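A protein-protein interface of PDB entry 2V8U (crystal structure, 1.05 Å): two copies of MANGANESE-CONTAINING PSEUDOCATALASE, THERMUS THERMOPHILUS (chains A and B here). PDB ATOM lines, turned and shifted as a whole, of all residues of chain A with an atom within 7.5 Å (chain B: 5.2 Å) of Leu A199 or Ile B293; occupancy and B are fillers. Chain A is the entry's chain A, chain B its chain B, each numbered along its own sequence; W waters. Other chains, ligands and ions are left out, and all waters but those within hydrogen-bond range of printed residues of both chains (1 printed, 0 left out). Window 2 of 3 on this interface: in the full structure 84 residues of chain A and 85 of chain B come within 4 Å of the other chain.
No position is printed for both chains.
Of the 10 pairs that touch across the chains among the printed residues, none has its exchanged pair printed and touching as well.
Ala A55 touches Tyr B291 (CB to CE1, 3.6 Å).
Ala B294 touches Ala A55.
Leu A56 touches Leu B290.
CD1 of Tyr B291 touches CG of Leu A56, 3.8 Å away.
Pro A58 touches Leu B297 (CG to CD1, 3.97 Å).
OH of Tyr A59 touches CG2 of Ile B293, 3.6 Å away.
Leu B297 touches Tyr A59.
O of Ser A198 touches CG2 of Ile B293, 3.5 Å away.
Leu A199 touches Leu B290.
O of Leu A199 touches CD1 of Ile B293, at 3.9 Å.
The side-chain hydroxyl (OH) of Tyr A59 lies within hydrogen-bond range of the side-chain hydroxyl (OG) of Ser A198 (2.8 Å).
O of Ala A195 lies within hydrogen-bond range of OG of Ser A198 (2.8 Å).
Of the 9 printed residues of chain B, 5 touch a printed residue of chain A.
Printed residues of chain B that touch a printed residue of chain A: Leu B290, Tyr B291, Ile B293, Ala B294 and Leu B297.
Of the 19 printed residues of chain A, 6 touch a printed residue of chain B.
Among the printed residues, 10 pairs touch across the chains.
Among the printed residues, no Asp or Glu carboxylate lies within 4 Å of a Lys or Arg side-chain nitrogen of the other chain.
Of the printed residues of chain B, Ala A55 touches Tyr B291 (3.6 Å) and Ala B294 (3.4 Å).
Printed residues of chain B within 4 Å of Ser A198: Ile B293.
Of chain B, only Leu B290 (3.9 Å) and Ile B293 (3.9 Å) come within 4 Å of Leu A199.
Of the printed residues of chain A, Ile B293 touches Tyr A59 (3.6 Å), Ser A198 (3.5 Å) and Leu A199 (3.9 Å).
The nearest printed residue of chain B that does not touch Pro A58 is Ala B294 (4.4 Å).
Water W1 lies within hydrogen-bond range of the backbone carbonyl oxygen of Ala A55 (2.7 Å) and the backbone carbonyl oxygen of Tyr B291 (2.8 Å).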
ATOM      1  N   ALA A  55     -20.298  34.119 -20.124  1.00  0.00           N
ATOM      2  CA  ALA A  55     -20.626  32.702 -20.037  1.00  0.00           C
ATOM      3  C   ALA A  55     -19.423  31.797 -20.259  1.00  0.00           C
ATOM      4  O   ALA A  55     -19.367  30.676 -19.716  1.00  0.00           O
ATOM      5  CB  ALA A  55     -21.733  32.354 -21.008  1.00  0.00           C
ATOM      6  N   LEU A  56     -18.446  32.258 -21.036  1.00  0.00           N
ATOM      7  CA  LEU A  56     -17.212  31.526 -21.310  1.00  0.00           C
ATOM      8  C   LEU A  56     -16.007  32.298 -20.756  1.00  0.00           C
ATOM      9  O   LEU A  56     -14.889  32.244 -21.294  1.00  0.00           O
ATOM     10  CB  LEU A  56     -17.048  31.255 -22.799  1.00  0.00           C
ATOM     11  CG  LEU A  56     -18.123  30.325 -23.361  1.00  0.00           C
ATOM     12  CD1 LEU A  56     -18.176  30.416 -24.876  1.00  0.00           C
ATOM     13  CD2 LEU A  56     -17.897  28.909 -22.908  1.00  0.00           C
ATOM     14  N   PRO A  58     -13.612  32.120 -18.425  1.00  0.00           N
ATOM     15  CA  PRO A  58     -12.220  31.670 -18.249  1.00  0.00           C
ATOM     16  C   PRO A  58     -11.447  31.698 -19.565  1.00  0.00           C
ATOM     17  O   PRO A  58     -10.250  32.027 -19.587  1.00  0.00           O
ATOM     18  CB  PRO A  58     -12.385  30.265 -17.666  1.00  0.00           C
ATOM     19  CG  PRO A  58     -13.752  30.314 -16.980  1.00  0.00           C
ATOM     20  CD  PRO A  58     -14.590  31.143 -17.902  1.00  0.00           C
ATOM     21  N   TYR A  59     -12.126  31.350 -20.649  1.00  0.00           N
ATOM     22  CA  TYR A  59     -11.496  31.309 -21.974  1.00  0.00           C
ATOM     23  C   TYR A  59     -11.296  32.706 -22.552  1.00  0.00           C
ATOM     24  O   TYR A  59     -10.275  32.980 -23.189  1.00  0.00           O
ATOM     25  CB  TYR A  59     -12.359  30.451 -22.925  1.00  0.00           C
ATOM     26  CG  TYR A  59     -12.629  29.082 -22.378  1.00  0.00           C
ATOM     27  CD1 TYR A  59     -11.694  28.071 -22.447  1.00  0.00           C
ATOM     28  CD2 TYR A  59     -13.802  28.795 -21.692  1.00  0.00           C
ATOM     29  CE1 TYR A  59     -11.892  26.855 -21.851  1.00  0.00           C
ATOM     30  CE2 TYR A  59     -14.014  27.574 -21.094  1.00  0.00           C
ATOM     31  CZ  TYR A  59     -13.056  26.594 -21.189  1.00  0.00           C
ATOM     32  OH  TYR A  59     -13.289  25.383 -20.598  1.00  0.00           O
ATOM     33  N   LEU A 144     -15.145  29.145 -30.732  1.00  0.00           N
ATOM     34  CA  LEU A 144     -14.103  29.098 -29.714  1.00  0.00           C
ATOM     35  C   LEU A 144     -13.113  27.945 -29.933  1.00  0.00           C
ATOM     36  O   LEU A 144     -11.898  28.154 -29.883  1.00  0.00           O
ATOM     37  CB  LEU A 144     -14.758  29.007 -28.335  1.00  0.00           C
ATOM     38  CG  LEU A 144     -13.780  28.927 -27.171  1.00  0.00           C
ATOM     39  CD1 LEU A 144     -12.793  30.084 -27.140  1.00  0.00           C
ATOM     40  CD2 LEU A 144     -14.541  28.800 -25.867  1.00  0.00           C
ATOM     41  N   ILE A 145     -13.630  26.723 -30.160  1.00  0.00           N
ATOM     42  CA  ILE A 145     -12.731  25.594 -30.296  1.00  0.00           C
ATOM     43  C   ILE A 145     -11.864  25.726 -31.539  1.00  0.00           C
ATOM     44  O   ILE A 145     -10.674  25.420 -31.522  1.00  0.00           O
ATOM     45  CB  ILE A 145     -13.505  24.269 -30.220  1.00  0.00           C
ATOM     46  CG1 ILE A 145     -14.026  24.062 -28.782  1.00  0.00           C
ATOM     47  CG2 ILE A 145     -12.649  23.096 -30.674  1.00  0.00           C
ATOM     48  CD1 ILE A 145     -15.096  23.007 -28.657  1.00  0.00           C
ATOM     49  N   LEU A 148      -9.168  28.188 -30.835  1.00  0.00           N
ATOM     50  CA  LEU A 148      -8.172  27.674 -29.931  1.00  0.00           C
ATOM     51  C   LEU A 148      -7.252  26.649 -30.597  1.00  0.00           C
ATOM     52  O   LEU A 148      -6.058  26.608 -30.315  1.00  0.00           O
ATOM     53  CB  LEU A 148      -8.799  27.077 -28.677  1.00  0.00           C
ATOM     54  CG  LEU A 148      -9.394  28.103 -27.698  1.00  0.00           C
ATOM     55  CD1 LEU A 148     -10.263  27.338 -26.669  1.00  0.00           C
ATOM     56  CD2 LEU A 148      -8.318  28.859 -27.000  1.00  0.00           C
ATOM     57  N   TYR A 192      -3.240  27.161 -24.255  1.00  0.00           N
ATOM     58  CA  TYR A 192      -4.248  26.832 -25.246  1.00  0.00           C
ATOM     59  C   TYR A 192      -4.484  25.326 -25.291  1.00  0.00           C
ATOM     60  O   TYR A 192      -5.639  24.897 -25.508  1.00  0.00           O
ATOM     61  CB  TYR A 192      -3.868  27.393 -26.623  1.00  0.00           C
ATOM     62  CG  TYR A 192      -3.858  28.910 -26.677  1.00  0.00           C
ATOM     63  CD1 TYR A 192      -4.864  29.660 -26.117  1.00  0.00           C
ATOM     64  CD2 TYR A 192      -2.846  29.588 -27.306  1.00  0.00           C
ATOM     65  CE1 TYR A 192      -4.875  31.035 -26.179  1.00  0.00           C
ATOM     66  CE2 TYR A 192      -2.829  30.975 -27.372  1.00  0.00           C
ATOM     67  CZ  TYR A 192      -3.861  31.701 -26.832  1.00  0.00           C
ATOM     68  OH  TYR A 192      -3.939  33.078 -26.847  1.00  0.00           O
ATOM     69  N   GLY A 193      -3.463  24.518 -25.062  1.00  0.00           N
ATOM     70  CA  GLY A 193      -3.647  23.089 -24.971  1.00  0.00           C
ATOM     71  C   GLY A 193      -4.536  22.685 -23.792  1.00  0.00           C
ATOM     72  O   GLY A 193      -5.426  21.859 -23.946  1.00  0.00           O
ATOM     73  N   LYS A 194      -4.307  23.302 -22.629  1.00  0.00           N
ATOM     74  CA  LYS A 194      -5.155  23.070 -21.473  1.00  0.00           C
ATOM     75  C   LYS A 194      -6.566  23.544 -21.728  1.00  0.00           C
ATOM     76  O   LYS A 194      -7.537  22.891 -21.305  1.00  0.00           O
ATOM     77  CB  LYS A 194      -4.560  23.762 -20.241  1.00  0.00           C
ATOM     78  CG  LYS A 194      -3.324  23.049 -19.672  1.00  0.00           C
ATOM     79  CD  LYS A 194      -2.653  23.852 -18.578  1.00  0.00           C
ATOM     80  CE  LYS A 194      -1.378  23.246 -18.048  1.00  0.00           C
ATOM     81  NZ  LYS A 194      -1.642  21.999 -17.257  1.00  0.00           N
ATOM     82  N   ALA A 195      -6.749  24.667 -22.415  1.00  0.00           N
ATOM     83  CA  ALA A 195      -8.086  25.136 -22.756  1.00  0.00           C
ATOM     84  C   ALA A 195      -8.794  24.098 -23.630  1.00  0.00           C
ATOM     85  O   ALA A 195      -9.968  23.770 -23.411  1.00  0.00           O
ATOM     86  CB  ALA A 195      -8.017  26.495 -23.459  1.00  0.00           C
ATOM     87  N   LEU A 196      -8.097  23.595 -24.660  1.00  0.00           N
ATOM     88  CA  LEU A 196      -8.687  22.555 -25.508  1.00  0.00           C
ATOM     89  C   LEU A 196      -8.991  21.284 -24.721  1.00  0.00           C
ATOM     90  O   LEU A 196     -10.033  20.666 -24.972  1.00  0.00           O
ATOM     91  CB  LEU A 196      -7.764  22.266 -26.691  1.00  0.00           C
ATOM     92  CG  LEU A 196      -7.762  23.360 -27.763  1.00  0.00           C
ATOM     93  CD1 LEU A 196      -6.551  23.242 -28.669  1.00  0.00           C
ATOM     94  CD2 LEU A 196      -9.033  23.316 -28.578  1.00  0.00           C
ATOM     95  N   GLU A 197      -8.131  20.888 -23.812  1.00  0.00           N
ATOM     96  CA  GLU A 197      -8.415  19.710 -22.998  1.00  0.00           C
ATOM     97  C   GLU A 197      -9.713  19.873 -22.223  1.00  0.00           C
ATOM     98  O   GLU A 197     -10.552  18.985 -22.141  1.00  0.00           O
ATOM     99  CB  GLU A 197      -7.217  19.534 -21.958  1.00  0.00           C
ATOM    100  CG  GLU A 197      -5.919  19.027 -22.600  1.00  0.00           C
ATOM    101  CD  GLU A 197      -4.636  19.020 -21.804  1.00  0.00           C
ATOM    102  OE1 GLU A 197      -4.536  19.650 -20.702  1.00  0.00           O
ATOM    103  OE2 GLU A 197      -3.669  18.368 -22.359  1.00  0.00           O
ATOM    104  N   SER A 198      -9.918  21.054 -21.653  1.00  0.00           N
ATOM    105  CA  SER A 198     -11.117  21.317 -20.861  1.00  0.00           C
ATOM    106  C   SER A 198     -12.369  21.288 -21.730  1.00  0.00           C
ATOM    107  O   SER A 198     -13.413  20.835 -21.295  1.00  0.00           O
ATOM    108  CB  SER A 198     -10.931  22.651 -20.134  1.00  0.00           C
ATOM    109  OG  SER A 198     -11.050  23.749 -20.877  1.00  0.00           O
ATOM    110  N   LEU A 199     -12.292  21.791 -22.950  1.00  0.00           N
ATOM    111  CA  LEU A 199     -13.455  21.894 -23.814  1.00  0.00           C
ATOM    112  C   LEU A 199     -13.771  20.649 -24.613  1.00  0.00           C
ATOM    113  O   LEU A 199     -14.915  20.478 -25.039  1.00  0.00           O
ATOM    114  CB  LEU A 199     -13.279  23.060 -24.788  1.00  0.00           C
ATOM    115  CG  LEU A 199     -13.280  24.424 -24.163  1.00  0.00           C
ATOM    116  CD1 LEU A 199     -12.698  25.452 -25.138  1.00  0.00           C
ATOM    117  CD2 LEU A 199     -14.687  24.838 -23.731  1.00  0.00           C
ATOM    118  N   THR A 200     -12.780  19.797 -24.841  1.00  0.00           N
ATOM    119  CA  THR A 200     -12.889  18.696 -25.789  1.00  0.00           C
ATOM    120  C   THR A 200     -12.519  17.340 -25.212  1.00  0.00           C
ATOM    121  O   THR A 200     -12.823  16.304 -25.838  1.00  0.00           O
ATOM    122  CB  THR A 200     -12.024  18.911 -27.050  1.00  0.00           C
ATOM    123  OG1 THR A 200     -10.648  18.683 -26.758  1.00  0.00           O
ATOM    124  CG2 THR A 200     -12.223  20.283 -27.693  1.00  0.00           C
ATOM    125  N   GLY A 201     -11.755  17.296 -24.128  1.00  0.00           N
ATOM    126  CA  GLY A 201     -11.255  16.057 -23.603  1.00  0.00           C
ATOM    127  C   GLY A 201     -10.040  15.496 -24.300  1.00  0.00           C
ATOM    128  O   GLY A 201      -9.498  14.500 -23.844  1.00  0.00           O
ATOM    129  N   VAL A 202      -9.550  16.140 -25.343  1.00  0.00           N
ATOM    130  CA  VAL A 202      -8.390  15.679 -26.086  1.00  0.00           C
ATOM    131  C   VAL A 202      -7.149  16.240 -25.396  1.00  0.00           C
ATOM    132  O   VAL A 202      -7.080  17.449 -25.130  1.00  0.00           O
ATOM    133  CB  VAL A 202      -8.474  16.141 -27.567  1.00  0.00           C
ATOM    134  CG1 VAL A 202      -7.217  15.753 -28.316  1.00  0.00           C
ATOM    135  CG2 VAL A 202      -9.742  15.562 -28.218  1.00  0.00           C
ATOM    136  N   ILE A 247      -8.036  27.627 -15.895  1.00  0.00           N
ATOM    137  CA  ILE A 247      -7.434  26.893 -17.020  1.00  0.00           C
ATOM    138  C   ILE A 247      -5.938  26.697 -16.779  1.00  0.00           C
ATOM    139  O   ILE A 247      -5.396  25.608 -17.002  1.00  0.00           O
ATOM    140  CB  ILE A 247      -7.702  27.596 -18.350  1.00  0.00           C
ATOM    141  CG1 ILE A 247      -9.190  27.630 -18.668  1.00  0.00           C
ATOM    142  CG2 ILE A 247      -6.913  26.896 -19.471  1.00  0.00           C
ATOM    143  CD1 ILE A 247      -9.519  28.630 -19.755  1.00  0.00           C
ATOM    144  N   GLU B 289     -23.473  23.120 -23.900  1.00  0.00           N
ATOM    145  CA  GLU B 289     -22.509  22.242 -23.235  1.00  0.00           C
ATOM    146  C   GLU B 289     -21.242  23.009 -22.855  1.00  0.00           C
ATOM    147  O   GLU B 289     -20.701  22.798 -21.754  1.00  0.00           O
ATOM    148  CB  GLU B 289     -22.139  21.088 -24.148  1.00  0.00           C
ATOM    149  CG  GLU B 289     -21.127  20.166 -23.521  1.00  0.00           C
ATOM    150  CD  GLU B 289     -20.527  19.101 -24.427  1.00  0.00           C
ATOM    151  OE1 GLU B 289     -20.494  19.188 -25.676  1.00  0.00           O
ATOM    152  OE2 GLU B 289     -20.033  18.106 -23.864  1.00  0.00           O
ATOM    153  N   LEU B 290     -20.749  23.883 -23.712  1.00  0.00           N
ATOM    154  CA  LEU B 290     -19.541  24.644 -23.346  1.00  0.00           C
ATOM    155  C   LEU B 290     -19.804  25.562 -22.154  1.00  0.00           C
ATOM    156  O   LEU B 290     -18.947  25.727 -21.301  1.00  0.00           O
ATOM    157  CB  LEU B 290     -19.014  25.448 -24.520  1.00  0.00           C
ATOM    158  CG  LEU B 290     -18.630  24.628 -25.774  1.00  0.00           C
ATOM    159  CD1 LEU B 290     -17.856  25.489 -26.757  1.00  0.00           C
ATOM    160  CD2 LEU B 290     -17.889  23.372 -25.467  1.00  0.00           C
ATOM    161  N   TYR B 291     -20.991  26.173 -22.111  1.00  0.00           N
ATOM    162  CA  TYR B 291     -21.327  26.984 -20.946  1.00  0.00           C
ATOM    163  C   TYR B 291     -21.347  26.164 -19.669  1.00  0.00           C
ATOM    164  O   TYR B 291     -20.926  26.659 -18.616  1.00  0.00           O
ATOM    165  CB  TYR B 291     -22.685  27.652 -21.137  1.00  0.00           C
ATOM    166  CG  TYR B 291     -22.787  28.666 -22.262  1.00  0.00           C
ATOM    167  CD1 TYR B 291     -21.691  29.264 -22.843  1.00  0.00           C
ATOM    168  CD2 TYR B 291     -24.051  28.982 -22.777  1.00  0.00           C
ATOM    169  CE1 TYR B 291     -21.859  30.228 -23.861  1.00  0.00           C
ATOM    170  CE2 TYR B 291     -24.205  29.926 -23.781  1.00  0.00           C
ATOM    171  CZ  TYR B 291     -23.098  30.527 -24.343  1.00  0.00           C
ATOM    172  OH  TYR B 291     -23.214  31.466 -25.340  1.00  0.00           O
ATOM    173  N   GLU B 292     -21.794  24.935 -19.736  1.00  0.00           N
ATOM    174  CA  GLU B 292     -21.795  24.066 -18.556  1.00  0.00           C
ATOM    175  C   GLU B 292     -20.368  23.709 -18.139  1.00  0.00           C
ATOM    176  O   GLU B 292     -20.045  23.676 -16.955  1.00  0.00           O
ATOM    177  CB  GLU B 292     -22.573  22.770 -18.833  1.00  0.00           C
ATOM    178  CG  GLU B 292     -24.092  22.919 -18.984  1.00  0.00           C
ATOM    179  CD  GLU B 292     -24.856  23.629 -17.855  1.00  0.00           C
ATOM    180  OE1 GLU B 292     -24.305  23.993 -16.787  1.00  0.00           O
ATOM    181  OE2 GLU B 292     -26.078  23.840 -18.049  1.00  0.00           O
ATOM    182  N   ILE B 293     -19.486  23.431 -19.117  1.00  0.00           N
ATOM    183  CA  ILE B 293     -18.094  23.194 -18.809  1.00  0.00           C
ATOM    184  C   ILE B 293     -17.502  24.395 -18.099  1.00  0.00           C
ATOM    185  O   ILE B 293     -16.791  24.242 -17.081  1.00  0.00           O
ATOM    186  CB  ILE B 293     -17.328  22.827 -20.098  1.00  0.00           C
ATOM    187  CG1 ILE B 293     -17.770  21.452 -20.613  1.00  0.00           C
ATOM    188  CG2 ILE B 293     -15.819  22.893 -19.881  1.00  0.00           C
ATOM    189  CD1 ILE B 293     -17.265  21.129 -21.998  1.00  0.00           C
ATOM    190  N   ALA B 294     -17.730  25.593 -18.630  1.00  0.00           N
ATOM    191  CA  ALA B 294     -17.190  26.793 -18.017  1.00  0.00           C
ATOM    192  C   ALA B 294     -17.697  26.967 -16.604  1.00  0.00           C
ATOM    193  O   ALA B 294     -16.943  27.298 -15.709  1.00  0.00           O
ATOM    194  CB  ALA B 294     -17.502  28.009 -18.862  1.00  0.00           C
ATOM    195  N   LYS B 295     -18.992  26.764 -16.371  1.00  0.00           N
ATOM    196  CA  LYS B 295     -19.581  26.883 -15.042  1.00  0.00           C
ATOM    197  C   LYS B 295     -18.909  25.932 -14.075  1.00  0.00           C
ATOM    198  O   LYS B 295     -18.602  26.304 -12.936  1.00  0.00           O
ATOM    199  CB  LYS B 295     -21.084  26.651 -15.145  1.00  0.00           C
ATOM    200  CG  LYS B 295     -21.780  26.814 -13.856  1.00  0.00           C
ATOM    201  CD  LYS B 295     -23.251  26.699 -14.034  1.00  0.00           C
ATOM    202  CE  LYS B 295     -23.951  27.025 -12.747  1.00  0.00           C
ATOM    203  NZ  LYS B 295     -25.403  26.727 -12.876  1.00  0.00           N
ATOM    204  N   LYS B 296     -18.693  24.697 -14.509  1.00  0.00           N
ATOM    205  CA  LYS B 296     -18.090  23.720 -13.635  1.00  0.00           C
ATOM    206  C   LYS B 296     -16.633  24.047 -13.273  1.00  0.00           C
ATOM    207  O   LYS B 296     -16.137  23.632 -12.219  1.00  0.00           O
ATOM    208  CB  LYS B 296     -18.219  22.355 -14.268  1.00  0.00           C
ATOM    209  CG  LYS B 296     -19.597  21.761 -14.159  1.00  0.00           C
ATOM    210  CD  LYS B 296     -19.597  20.302 -14.607  1.00  0.00           C
ATOM    211  CE  LYS B 296     -20.994  19.680 -14.584  1.00  0.00           C
ATOM    212  NZ  LYS B 296     -21.875  20.172 -15.644  1.00  0.00           N
ATOM    213  N   LEU B 297     -15.938  24.819 -14.103  1.00  0.00           N
ATOM    214  CA  LEU B 297     -14.566  25.233 -13.766  1.00  0.00           C
ATOM    215  C   LEU B 297     -14.498  26.018 -12.509  1.00  0.00           C
ATOM    216  O   LEU B 297     -13.445  26.006 -11.845  1.00  0.00           O
ATOM    217  CB  LEU B 297     -13.936  26.067 -14.871  1.00  0.00           C
ATOM    218  CG  LEU B 297     -13.575  25.384 -16.175  1.00  0.00           C
ATOM    219  CD1 LEU B 297     -13.125  26.400 -17.146  1.00  0.00           C
ATOM    220  CD2 LEU B 297     -12.533  24.324 -16.033  1.00  0.00           C
HETATM  221  O   HOH W   1     -21.187  29.416 -18.189  1.00  0.00           O
